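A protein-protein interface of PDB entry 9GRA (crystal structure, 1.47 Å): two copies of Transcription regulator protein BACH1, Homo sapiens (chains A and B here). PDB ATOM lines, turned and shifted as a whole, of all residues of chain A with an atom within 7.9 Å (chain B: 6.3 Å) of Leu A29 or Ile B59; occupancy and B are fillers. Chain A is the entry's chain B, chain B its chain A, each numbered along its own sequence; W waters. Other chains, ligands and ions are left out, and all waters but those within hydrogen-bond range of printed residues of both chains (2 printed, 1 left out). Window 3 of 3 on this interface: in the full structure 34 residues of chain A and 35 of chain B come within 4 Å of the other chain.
Printed residues of chain B within 4 Å of Ser A19: Ala B50 (3.6 Å). Printed residues of chain B within 4 Å of Gln A23: Ser B46 (3.1 Å). Of chain B, only Ala B49 (3.7 Å) and Ile B59 (3.5 Å) come within 4 Å of Leu A29. Printed residues of chain B within 4 Å of His A44: Ser B46. Of the printed residues of chain A, His B44 touches Ser A46. Ile B59 touches just one residue of chain A: Leu A29. The nearest residue of chain A that does not touch Ile B59 is Val A28 (7.1 Å).
N of Val A28 lies within hydrogen-bond range of O of Gln A23, at 2.9 Å. A ring nitrogen (NE2) of His A44 sits at hydrogen-bond distance from the side-chain amide oxygen (OE1) of Gln A23 (2.9 Å). The backbone carbonyl oxygen (O) of Leu A29 sits close to a ring nitrogen (NE2) of His A44 (3.4 Å). The side-chain hydroxyl (OH) of Tyr A88 lies within hydrogen-bond range of a ring nitrogen (ND1) of His A44, at 2.7 Å.
Among the printed residues, pairs that only touch across the chains: Ser A46 with His B44 (3.4 Å), His A44 with Ser B46 (3.5 Å), Leu A29 with Ile B59 (3.5 Å), Ser A19 with Ala B50 (3.6 Å), Leu A20 with Ser B46 (3.6 Å) and Leu A29 with Ala B49 (3.7 Å).
Hydrophobic or aromatic side chains of chain A that line the printed part of chain B: Leu A20, Leu A29 and His A44. Along chain A the printed residues that touch a printed residue of chain B span positions 19 to 46. Of the 19 printed residues of chain B, 5 touch a printed residue of chain A. Printed residues of chain B that touch a printed residue of chain A: His B44, Ser B46, Ala B49, Ala B50 and Ile B59. Hydrophobic or aromatic side chains of chain B that line the printed part of chain A: His B44, Ala B49, Ala B50 and Ile B59.
His A44 touches Ser B46, and with the chains exchanged Ser A46 touches His B44. Positions printed for both chains: 32, 44, 45 and 46.
Water W2 lies within hydrogen-bond range of the side-chain hydroxyl of Ser A19 (2.7 Å) and the backbone carbonyl oxygen of Ala B50 (2.7 Å). Water W1 bridges the side-chain hydroxyl (OG) of Ser B46 (2.9 Å) and the side-chain hydroxyl (OG) of Ser A46 (2.9 Å).
The backbone carbonyl oxygen of Ser B46 sits at hydrogen-bond distance from the side-chain amide nitrogen of Gln A23.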
ATOM      1  N   SER A  19      21.850   6.440  20.537  1.00  0.00           N
ATOM      2  CA  SER A  19      22.094   7.239  19.354  1.00  0.00           C
ATOM      3  C   SER A  19      21.650   6.507  18.093  1.00  0.00           C
ATOM      4  O   SER A  19      21.027   7.100  17.205  1.00  0.00           O
ATOM      5  CB  SER A  19      23.574   7.584  19.282  1.00  0.00           C
ATOM      6  OG  SER A  19      23.957   8.377  20.405  1.00  0.00           O
ATOM      7  N   LEU A  20      21.923   5.201  18.005  1.00  0.00           N
ATOM      8  CA  LEU A  20      21.466   4.443  16.846  1.00  0.00           C
ATOM      9  C   LEU A  20      19.935   4.445  16.765  1.00  0.00           C
ATOM     10  O   LEU A  20      19.360   4.533  15.661  1.00  0.00           O
ATOM     11  CB  LEU A  20      21.985   3.004  16.937  1.00  0.00           C
ATOM     12  CG  LEU A  20      23.488   2.871  16.786  1.00  0.00           C
ATOM     13  CD1 LEU A  20      23.935   1.413  17.065  1.00  0.00           C
ATOM     14  CD2 LEU A  20      23.950   3.380  15.421  1.00  0.00           C
ATOM     15  N   GLN A  23      18.929   7.821  15.329  1.00  0.00           N
ATOM     16  CA  GLN A  23      19.123   7.769  13.871  1.00  0.00           C
ATOM     17  C   GLN A  23      17.985   7.021  13.185  1.00  0.00           C
ATOM     18  O   GLN A  23      17.430   7.451  12.160  1.00  0.00           O
ATOM     19  CB  GLN A  23      20.439   7.067  13.568  1.00  0.00           C
ATOM     20  CG  GLN A  23      21.599   7.923  14.015  1.00  0.00           C
ATOM     21  CD  GLN A  23      22.925   7.177  13.941  1.00  0.00           C
ATOM     22  OE1 GLN A  23      23.033   6.136  13.293  1.00  0.00           O
ATOM     23  NE2 GLN A  23      23.944   7.683  14.656  1.00  0.00           N
ATOM     24  N   ARG A  24      17.621   5.874  13.750  1.00  0.00           N
ATOM     25  CA  ARG A  24      16.579   5.068  13.128  1.00  0.00           C
ATOM     26  C   ARG A  24      15.257   5.826  13.087  1.00  0.00           C
ATOM     27  O   ARG A  24      14.602   5.875  12.043  1.00  0.00           O
ATOM     28  CB  ARG A  24      16.430   3.755  13.915  1.00  0.00           C
ATOM     29  CG  ARG A  24      15.189   2.921  13.492  1.00  0.00           C
ATOM     30  CD  ARG A  24      15.017   1.743  14.355  1.00  0.00           C
ATOM     31  NE  ARG A  24      14.433   2.089  15.652  1.00  0.00           N
ATOM     32  CZ  ARG A  24      13.126   2.134  15.890  1.00  0.00           C
ATOM     33  NH1 ARG A  24      12.239   1.846  14.945  1.00  0.00           N
ATOM     34  NH2 ARG A  24      12.701   2.455  17.108  1.00  0.00           N
ATOM     35  N   LYS A  26      14.657   9.043  13.282  1.00  0.00           N
ATOM     36  CA  LYS A  26      14.705  10.235  12.480  1.00  0.00           C
ATOM     37  C   LYS A  26      15.127   9.939  11.043  1.00  0.00           C
ATOM     38  O   LYS A  26      15.248  10.891  10.247  1.00  0.00           O
ATOM     39  CB  LYS A  26      15.573  11.272  13.185  1.00  0.00           C
ATOM     40  CG  LYS A  26      14.924  11.766  14.507  1.00  0.00           C
ATOM     41  CD  LYS A  26      15.824  12.729  15.224  1.00  0.00           C
ATOM     42  CE  LYS A  26      15.033  13.332  16.402  1.00  0.00           C
ATOM     43  NZ  LYS A  26      14.497  12.332  17.426  1.00  0.00           N
ATOM     44  N   ASP A  27      15.369   8.658  10.720  1.00  0.00           N
ATOM     45  CA  ASP A  27      15.777   8.210   9.387  1.00  0.00           C
ATOM     46  C   ASP A  27      16.995   8.958   8.895  1.00  0.00           C
ATOM     47  O   ASP A  27      16.995   9.505   7.773  1.00  0.00           O
ATOM     48  CB  ASP A  27      14.641   8.288   8.350  1.00  0.00           C
ATOM     49  CG  ASP A  27      14.998   7.579   7.035  1.00  0.00           C
ATOM     50  OD1 ASP A  27      16.006   6.790   7.051  1.00  0.00           O
ATOM     51  OD2 ASP A  27      14.284   7.794   6.041  1.00  0.00           O
ATOM     52  N   VAL A  28      18.056   8.931   9.705  1.00  0.00           N
ATOM     53  CA  VAL A  28      19.325   9.436   9.214  1.00  0.00           C
ATOM     54  C   VAL A  28      20.384   8.372   9.474  1.00  0.00           C
ATOM     55  O   VAL A  28      20.331   7.633  10.459  1.00  0.00           O
ATOM     56  CB  VAL A  28      19.645  10.792   9.865  1.00  0.00           C
ATOM     57  CG1 VAL A  28      19.858  10.654  11.336  1.00  0.00           C
ATOM     58  CG2 VAL A  28      20.792  11.538   9.135  1.00  0.00           C
ATOM     59  N   LEU A  29      21.333   8.285   8.562  1.00  0.00           N
ATOM     60  CA  LEU A  29      22.452   7.329   8.656  1.00  0.00           C
ATOM     61  C   LEU A  29      22.011   5.881   8.668  1.00  0.00           C
ATOM     62  O   LEU A  29      22.764   5.002   9.128  1.00  0.00           O
ATOM     63  CB  LEU A  29      23.363   7.626   9.864  1.00  0.00           C
ATOM     64  CG  LEU A  29      23.850   9.087   9.790  1.00  0.00           C
ATOM     65  CD1 LEU A  29      24.732   9.259  10.979  1.00  0.00           C
ATOM     66  CD2 LEU A  29      24.613   9.361   8.527  1.00  0.00           C
ATOM     67  N   CYS A  30      20.803   5.602   8.180  1.00  0.00           N
ATOM     68  CA  CYS A  30      20.398   4.200   8.075  1.00  0.00           C
ATOM     69  C   CYS A  30      20.715   3.746   6.662  1.00  0.00           C
ATOM     70  O   CYS A  30      21.070   4.528   5.778  1.00  0.00           O
ATOM     71  CB  CYS A  30      18.883   4.132   8.260  1.00  0.00           C
ATOM     72  SG  CYS A  30      18.376   4.423   9.952  1.00  0.00           S
ATOM     73  N   ASP A  31      20.542   2.441   6.434  1.00  0.00           N
ATOM     74  CA  ASP A  31      21.083   1.849   5.216  1.00  0.00           C
ATOM     75  C   ASP A  31      20.263   0.647   4.755  1.00  0.00           C
ATOM     76  O   ASP A  31      20.624   0.003   3.764  1.00  0.00           O
ATOM     77  CB  ASP A  31      22.538   1.429   5.454  1.00  0.00           C
ATOM     78  CG  ASP A  31      22.684   0.496   6.615  1.00  0.00           C
ATOM     79  OD1 ASP A  31      22.319  -0.664   6.416  1.00  0.00           O
ATOM     80  OD2 ASP A  31      23.167   0.889   7.673  1.00  0.00           O
ATOM     81  N   VAL A  32      19.150   0.342   5.400  1.00  0.00           N
ATOM     82  CA  VAL A  32      18.318  -0.737   4.935  1.00  0.00           C
ATOM     83  C   VAL A  32      16.873  -0.316   5.147  1.00  0.00           C
ATOM     84  O   VAL A  32      16.534   0.336   6.144  1.00  0.00           O
ATOM     85  CB  VAL A  32      18.691  -2.077   5.607  1.00  0.00           C
ATOM     86  CG1 VAL A  32      18.509  -2.033   7.093  1.00  0.00           C
ATOM     87  CG2 VAL A  32      17.794  -3.173   5.088  1.00  0.00           C
ATOM     88  N   ARG A  42      12.959   1.716   8.644  1.00  0.00           N
ATOM     89  CA  ARG A  42      14.362   1.974   8.350  1.00  0.00           C
ATOM     90  C   ARG A  42      15.226   1.426   9.478  1.00  0.00           C
ATOM     91  O   ARG A  42      14.791   1.346  10.632  1.00  0.00           O
ATOM     92  CB  ARG A  42      14.601   3.488   8.187  1.00  0.00           C
ATOM     93  CG  ARG A  42      13.937   3.976   6.931  1.00  0.00           C
ATOM     94  CD  ARG A  42      14.692   3.591   5.659  1.00  0.00           C
ATOM     95  NE  ARG A  42      15.967   4.338   5.606  1.00  0.00           N
ATOM     96  CZ  ARG A  42      16.957   4.025   4.770  1.00  0.00           C
ATOM     97  NH1 ARG A  42      16.853   2.998   3.943  1.00  0.00           N
ATOM     98  NH2 ARG A  42      18.079   4.771   4.753  1.00  0.00           N
ATOM     99  N   ALA A  43      16.432   0.955   9.132  1.00  0.00           N
ATOM    100  CA  ALA A  43      17.334   0.427  10.150  1.00  0.00           C
ATOM    101  C   ALA A  43      18.737   0.422   9.576  1.00  0.00           C
ATOM    102  O   ALA A  43      18.996   0.927   8.486  1.00  0.00           O
ATOM    103  CB  ALA A  43      16.956  -0.977  10.633  1.00  0.00           C
ATOM    104  N   HIS A  44      19.673  -0.039  10.406  1.00  0.00           N
ATOM    105  CA  HIS A  44      21.054  -0.247   9.998  1.00  0.00           C
ATOM    106  C   HIS A  44      21.272  -1.761   9.861  1.00  0.00           C
ATOM    107  O   HIS A  44      20.971  -2.528  10.782  1.00  0.00           O
ATOM    108  CB  HIS A  44      22.009   0.206  11.133  1.00  0.00           C
ATOM    109  CG  HIS A  44      21.751   1.621  11.634  1.00  0.00           C
ATOM    110  ND1 HIS A  44      20.800   1.884  12.598  1.00  0.00           N
ATOM    111  CD2 HIS A  44      22.387   2.807  11.381  1.00  0.00           C
ATOM    112  CE1 HIS A  44      20.778   3.189  12.861  1.00  0.00           C
ATOM    113  NE2 HIS A  44      21.753   3.772  12.164  1.00  0.00           N
ATOM    114  N   ARG A  45      21.823  -2.177   8.729  1.00  0.00           N
ATOM    115  CA  ARG A  45      21.974  -3.629   8.504  1.00  0.00           C
ATOM    116  C   ARG A  45      22.907  -4.257   9.525  1.00  0.00           C
ATOM    117  O   ARG A  45      22.727  -5.448   9.907  1.00  0.00           O
ATOM    118  CB  ARG A  45      22.457  -3.879   7.067  1.00  0.00           C
ATOM    119  CG  ARG A  45      23.910  -3.512   6.775  1.00  0.00           C
ATOM    120  CD  ARG A  45      24.159  -3.597   5.270  1.00  0.00           C
ATOM    121  NE  ARG A  45      23.482  -2.524   4.551  1.00  0.00           N
ATOM    122  CZ  ARG A  45      23.549  -2.364   3.242  1.00  0.00           C
ATOM    123  NH1 ARG A  45      24.257  -3.197   2.499  1.00  0.00           N
ATOM    124  NH2 ARG A  45      22.994  -1.276   2.691  1.00  0.00           N
ATOM    125  N   SER A  46      23.887  -3.481  10.021  1.00  0.00           N
ATOM    126  CA  SER A  46      24.839  -3.989  11.000  1.00  0.00           C
ATOM    127  C   SER A  46      24.110  -4.385  12.282  1.00  0.00           C
ATOM    128  O   SER A  46      24.373  -5.440  12.864  1.00  0.00           O
ATOM    129  CB  SER A  46      25.905  -2.939  11.298  1.00  0.00           C
ATOM    130  OG  SER A  46      25.277  -1.714  11.645  1.00  0.00           O
ATOM    131  N   GLU A  66      22.069   1.261  -0.599  1.00  0.00           N
ATOM    132  CA  GLU A  66      20.818   0.986   0.104  1.00  0.00           C
ATOM    133  C   GLU A  66      20.357  -0.430  -0.199  1.00  0.00           C
ATOM    134  O   GLU A  66      20.462  -0.895  -1.337  1.00  0.00           O
ATOM    135  CB  GLU A  66      19.730   1.958  -0.341  1.00  0.00           C
ATOM    136  CG  GLU A  66      19.819   3.288   0.370  1.00  0.00           C
ATOM    137  CD  GLU A  66      19.420   3.160   1.826  1.00  0.00           C
ATOM    138  OE1 GLU A  66      18.730   2.165   2.176  1.00  0.00           O
ATOM    139  OE2 GLU A  66      19.789   4.046   2.621  1.00  0.00           O
ATOM    140  N   TYR A  88      16.607  -1.910  19.236  1.00  0.00           N
ATOM    141  CA  TYR A  88      17.224  -0.596  19.374  1.00  0.00           C
ATOM    142  C   TYR A  88      17.151   0.027  20.751  1.00  0.00           C
ATOM    143  O   TYR A  88      17.682   1.153  20.921  1.00  0.00           O
ATOM    144  CB  TYR A  88      16.639   0.332  18.318  1.00  0.00           C
ATOM    145  CG  TYR A  88      17.311   0.213  16.965  1.00  0.00           C
ATOM    146  CD1 TYR A  88      16.929  -0.764  16.042  1.00  0.00           C
ATOM    147  CD2 TYR A  88      18.332   1.055  16.600  1.00  0.00           C
ATOM    148  CE1 TYR A  88      17.547  -0.873  14.789  1.00  0.00           C
ATOM    149  CE2 TYR A  88      18.988   0.945  15.336  1.00  0.00           C
ATOM    150  CZ  TYR A  88      18.570  -0.023  14.453  1.00  0.00           C
ATOM    151  OH  TYR A  88      19.101  -0.153  13.202  1.00  0.00           O
ATOM    152  N   VAL B  32      32.438   2.801   6.155  1.00  0.00           N
ATOM    153  CA  VAL B  32      33.342   3.944   6.066  1.00  0.00           C
ATOM    154  C   VAL B  32      34.769   3.417   6.228  1.00  0.00           C
ATOM    155  O   VAL B  32      35.035   2.557   7.074  1.00  0.00           O
ATOM    156  CB  VAL B  32      32.959   5.057   7.067  1.00  0.00           C
ATOM    157  CG1 VAL B  32      33.001   4.544   8.513  1.00  0.00           C
ATOM    158  CG2 VAL B  32      33.880   6.256   6.921  1.00  0.00           C
ATOM    159  N   HIS B  44      31.646   1.749  11.031  1.00  0.00           N
ATOM    160  CA  HIS B  44      30.264   2.041  10.661  1.00  0.00           C
ATOM    161  C   HIS B  44      30.044   3.530  10.892  1.00  0.00           C
ATOM    162  O   HIS B  44      30.288   4.018  11.998  1.00  0.00           O
ATOM    163  CB  HIS B  44      29.274   1.293  11.582  1.00  0.00           C
ATOM    164  CG  HIS B  44      29.522  -0.185  11.666  1.00  0.00           C
ATOM    165  ND1 HIS B  44      30.434  -0.709  12.554  1.00  0.00           N
ATOM    166  CD2 HIS B  44      28.888  -1.240  11.078  1.00  0.00           C
ATOM    167  CE1 HIS B  44      30.416  -2.033  12.458  1.00  0.00           C
ATOM    168  NE2 HIS B  44      29.482  -2.380  11.586  1.00  0.00           N
ATOM    169  N   ARG B  45      29.557   4.223   9.861  1.00  0.00           N
ATOM    170  CA  ARG B  45      29.438   5.677  10.012  1.00  0.00           C
ATOM    171  C   ARG B  45      28.457   6.019  11.117  1.00  0.00           C
ATOM    172  O   ARG B  45      28.593   7.053  11.792  1.00  0.00           O
ATOM    173  CB  ARG B  45      29.052   6.348   8.695  1.00  0.00           C
ATOM    174  CG  ARG B  45      27.670   6.035   8.194  1.00  0.00           C
ATOM    175  CD  ARG B  45      27.464   6.561   6.785  1.00  0.00           C
ATOM    176  NE  ARG B  45      28.274   5.803   5.831  1.00  0.00           N
ATOM    177  CZ  ARG B  45      28.195   5.957   4.514  1.00  0.00           C
ATOM    178  NH1 ARG B  45      27.527   6.975   3.973  1.00  0.00           N
ATOM    179  NH2 ARG B  45      28.801   5.078   3.716  1.00  0.00           N
ATOM    180  N   SER B  46      27.451   5.168  11.310  1.00  0.00           N
ATOM    181  CA  SER B  46      26.483   5.418  12.365  1.00  0.00           C
ATOM    182  C   SER B  46      27.140   5.465  13.753  1.00  0.00           C
ATOM    183  O   SER B  46      26.768   6.298  14.612  1.00  0.00           O
ATOM    184  CB  SER B  46      25.378   4.368  12.262  1.00  0.00           C
ATOM    185  OG  SER B  46      25.988   3.083  12.328  1.00  0.00           O
ATOM    186  N   LEU B  48      30.516   5.947  14.375  1.00  0.00           N
ATOM    187  CA  LEU B  48      31.446   7.079  14.466  1.00  0.00           C
ATOM    188  C   LEU B  48      30.675   8.365  14.700  1.00  0.00           C
ATOM    189  O   LEU B  48      31.088   9.188  15.534  1.00  0.00           O
ATOM    190  CB  LEU B  48      32.237   7.252  13.181  1.00  0.00           C
ATOM    191  CG  LEU B  48      33.189   6.082  12.845  1.00  0.00           C
ATOM    192  CD1 LEU B  48      34.034   6.435  11.662  1.00  0.00           C
ATOM    193  CD2 LEU B  48      34.096   5.740  14.054  1.00  0.00           C
ATOM    194  N   ALA B  49      29.551   8.558  13.984  1.00  0.00           N
ATOM    195  CA  ALA B  49      28.765   9.793  14.177  1.00  0.00           C
ATOM    196  C   ALA B  49      28.174   9.872  15.582  1.00  0.00           C
ATOM    197  O   ALA B  49      28.031  10.973  16.159  1.00  0.00           O
ATOM    198  CB  ALA B  49      27.643   9.864  13.142  1.00  0.00           C
ATOM    199  N   ALA B  50      27.807   8.725  16.134  1.00  0.00           N
ATOM    200  CA  ALA B  50      27.283   8.693  17.491  1.00  0.00           C
ATOM    201  C   ALA B  50      28.333   9.117  18.499  1.00  0.00           C
ATOM    202  O   ALA B  50      27.988   9.635  19.564  1.00  0.00           O
ATOM    203  CB  ALA B  50      26.806   7.264  17.822  1.00  0.00           C
ATOM    204  N   TYR B  54      33.473  15.398  15.421  1.00  0.00           N
ATOM    205  CA  TYR B  54      34.301  15.579  14.230  1.00  0.00           C
ATOM    206  C   TYR B  54      33.833  14.662  13.111  1.00  0.00           C
ATOM    207  O   TYR B  54      33.644  15.086  11.963  1.00  0.00           O
ATOM    208  CB  TYR B  54      35.755  15.297  14.579  1.00  0.00           C
ATOM    209  CG  TYR B  54      36.707  15.476  13.456  1.00  0.00           C
ATOM    210  CD1 TYR B  54      36.905  14.434  12.538  1.00  0.00           C
ATOM    211  CD2 TYR B  54      37.437  16.661  13.302  1.00  0.00           C
ATOM    212  CE1 TYR B  54      37.805  14.599  11.470  1.00  0.00           C
ATOM    213  CE2 TYR B  54      38.344  16.818  12.247  1.00  0.00           C
ATOM    214  CZ  TYR B  54      38.545  15.756  11.371  1.00  0.00           C
ATOM    215  OH  TYR B  54      39.444  15.879  10.320  1.00  0.00           O
ATOM    216  N   PHE B  55      33.659  13.388  13.428  1.00  0.00           N
ATOM    217  CA  PHE B  55      33.193  12.473  12.384  1.00  0.00           C
ATOM    218  C   PHE B  55      31.763  12.789  11.955  1.00  0.00           C
ATOM    219  O   PHE B  55      31.446  12.760  10.773  1.00  0.00           O
ATOM    220  CB  PHE B  55      33.313  10.983  12.825  1.00  0.00           C
ATOM    221  CG  PHE B  55      34.665  10.419  12.672  1.00  0.00           C
ATOM    222  CD1 PHE B  55      35.238  10.297  11.422  1.00  0.00           C
ATOM    223  CD2 PHE B  55      35.387  10.029  13.764  1.00  0.00           C
ATOM    224  CE1 PHE B  55      36.514   9.798  11.276  1.00  0.00           C
ATOM    225  CE2 PHE B  55      36.686   9.522  13.621  1.00  0.00           C
ATOM    226  CZ  PHE B  55      37.245   9.397  12.372  1.00  0.00           C
ATOM    227  N   HIS B  56      30.913  13.177  12.906  1.00  0.00           N
ATOM    228  CA  HIS B  56      29.516  13.411  12.563  1.00  0.00           C
ATOM    229  C   HIS B  56      29.422  14.495  11.480  1.00  0.00           C
ATOM    230  O   HIS B  56      28.748  14.330  10.473  1.00  0.00           O
ATOM    231  CB  HIS B  56      28.742  13.750  13.853  1.00  0.00           C
ATOM    232  CG  HIS B  56      27.334  14.234  13.649  1.00  0.00           C
ATOM    233  ND1 HIS B  56      27.070  15.573  13.389  1.00  0.00           N
ATOM    234  CD2 HIS B  56      26.125  13.623  13.719  1.00  0.00           C
ATOM    235  CE1 HIS B  56      25.763  15.758  13.290  1.00  0.00           C
ATOM    236  NE2 HIS B  56      25.166  14.594  13.470  1.00  0.00           N
ATOM    237  N   SER B  57      30.181  15.584  11.629  1.00  0.00           N
ATOM    238  CA  SER B  57      30.157  16.651  10.629  1.00  0.00           C
ATOM    239  C   SER B  57      30.615  16.183   9.258  1.00  0.00           C
ATOM    240  O   SER B  57      30.281  16.832   8.260  1.00  0.00           O
ATOM    241  CB  SER B  57      31.098  17.750  11.109  1.00  0.00           C
ATOM    242  OG  SER B  57      30.641  18.140  12.399  1.00  0.00           O
ATOM    243  N   ARG B  58      31.417  15.101   9.190  1.00  0.00           N
ATOM    244  CA  ARG B  58      31.945  14.586   7.930  1.00  0.00           C
ATOM    245  C   ARG B  58      31.145  13.389   7.401  1.00  0.00           C
ATOM    246  O   ARG B  58      31.508  12.806   6.365  1.00  0.00           O
ATOM    247  CB  ARG B  58      33.414  14.198   8.114  1.00  0.00           C
ATOM    248  CG  ARG B  58      34.295  15.412   8.278  1.00  0.00           C
ATOM    249  CD  ARG B  58      35.640  15.012   8.883  1.00  0.00           C
ATOM    250  NE  ARG B  58      36.497  16.198   8.806  1.00  0.00           N
ATOM    251  CZ  ARG B  58      36.315  17.255   9.592  1.00  0.00           C
ATOM    252  NH1 ARG B  58      35.405  17.251  10.564  1.00  0.00           N
ATOM    253  NH2 ARG B  58      37.072  18.339   9.409  1.00  0.00           N
ATOM    254  N   ILE B  59      30.052  13.035   8.078  1.00  0.00           N
ATOM    255  CA  ILE B  59      29.253  11.871   7.758  1.00  0.00           C
ATOM    256  C   ILE B  59      27.856  12.263   7.333  1.00  0.00           C
ATOM    257  O   ILE B  59      27.335  11.745   6.341  1.00  0.00           O
ATOM    258  CB  ILE B  59      29.209  10.923   8.973  1.00  0.00           C
ATOM    259  CG1 ILE B  59      30.575  10.231   9.080  1.00  0.00           C
ATOM    260  CG2 ILE B  59      28.099   9.903   8.873  1.00  0.00           C
ATOM    261  CD1 ILE B  59      30.803   9.393  10.336  1.00  0.00           C
ATOM    262  N   VAL B  60      27.259  13.229   8.008  1.00  0.00           N
ATOM    263  CA  VAL B  60      25.860  13.516   7.715  1.00  0.00           C
ATOM    264  C   VAL B  60      25.774  14.137   6.327  1.00  0.00           C
ATOM    265  O   VAL B  60      26.646  14.925   5.915  1.00  0.00           O
ATOM    266  CB  VAL B  60      25.254  14.388   8.827  1.00  0.00           C
ATOM    267  CG1 VAL B  60      23.917  14.979   8.398  1.00  0.00           C
ATOM    268  CG2 VAL B  60      25.044  13.542  10.037  1.00  0.00           C
ATOM    269  N   GLY B  61      24.777  13.692   5.559  1.00  0.00           N
ATOM    270  CA  GLY B  61      24.577  14.186   4.209  1.00  0.00           C
ATOM    271  C   GLY B  61      25.541  13.701   3.153  1.00  0.00           C
ATOM    272  O   GLY B  61      25.443  14.153   2.003  1.00  0.00           O
ATOM    273  N   GLN B  62      26.451  12.784   3.492  1.00  0.00           N
ATOM    274  CA  GLN B  62      27.318  12.245   2.463  1.00  0.00           C
ATOM    275  C   GLN B  62      26.556  11.184   1.660  1.00  0.00           C
ATOM    276  O   GLN B  62      25.468  10.734   2.032  1.00  0.00           O
ATOM    277  CB  GLN B  62      28.527  11.586   3.118  1.00  0.00           C
ATOM    278  CG  GLN B  62      29.429  12.530   3.908  1.00  0.00           C
ATOM    279  CD  GLN B  62      30.185  13.497   3.054  1.00  0.00           C
ATOM    280  OE1 GLN B  62      30.603  13.182   1.922  1.00  0.00           O
ATOM    281  NE2 GLN B  62      30.381  14.715   3.583  1.00  0.00           N
ATOM    282  N   ALA B  63      27.150  10.765   0.552  1.00  0.00           N
ATOM    283  CA  ALA B  63      26.492   9.828  -0.348  1.00  0.00           C
ATOM    284  C   ALA B  63      26.245   8.472   0.338  1.00  0.00           C
ATOM    285  O   ALA B  63      26.892   8.122   1.325  1.00  0.00           O
ATOM    286  CB  ALA B  63      27.373   9.623  -1.578  1.00  0.00           C
ATOM    287  N   LEU B  67      32.012   5.486   2.176  1.00  0.00           N
ATOM    288  CA  LEU B  67      32.563   6.797   2.517  1.00  0.00           C
ATOM    289  C   LEU B  67      34.039   6.661   2.908  1.00  0.00           C
ATOM    290  O   LEU B  67      34.418   5.680   3.560  1.00  0.00           O
ATOM    291  CB  LEU B  67      31.751   7.338   3.686  1.00  0.00           C
ATOM    292  CG  LEU B  67      32.192   8.640   4.302  1.00  0.00           C
ATOM    293  CD1 LEU B  67      32.078   9.763   3.303  1.00  0.00           C
ATOM    294  CD2 LEU B  67      31.282   8.943   5.504  1.00  0.00           C
ATOM    295  N   ILE B  69      37.243   8.822   4.747  1.00  0.00           N
ATOM    296  CA  ILE B  69      37.654  10.007   5.507  1.00  0.00           C
ATOM    297  C   ILE B  69      39.136   9.899   5.814  1.00  0.00           C
ATOM    298  O   ILE B  69      39.582   8.880   6.345  1.00  0.00           O
ATOM    299  CB  ILE B  69      36.843  10.083   6.802  1.00  0.00           C
ATOM    300  CG1 ILE B  69      35.360  10.296   6.482  1.00  0.00           C
ATOM    301  CG2 ILE B  69      37.300  11.224   7.667  1.00  0.00           C
ATOM    302  CD1 ILE B  69      34.386  10.260   7.729  1.00  0.00           C
HETATM  303  O   HOH W   1      25.643   0.489  13.541  1.00  0.00           O
HETATM  304  O   HOH W   2      25.433  10.556  19.915  1.00  0.00           O
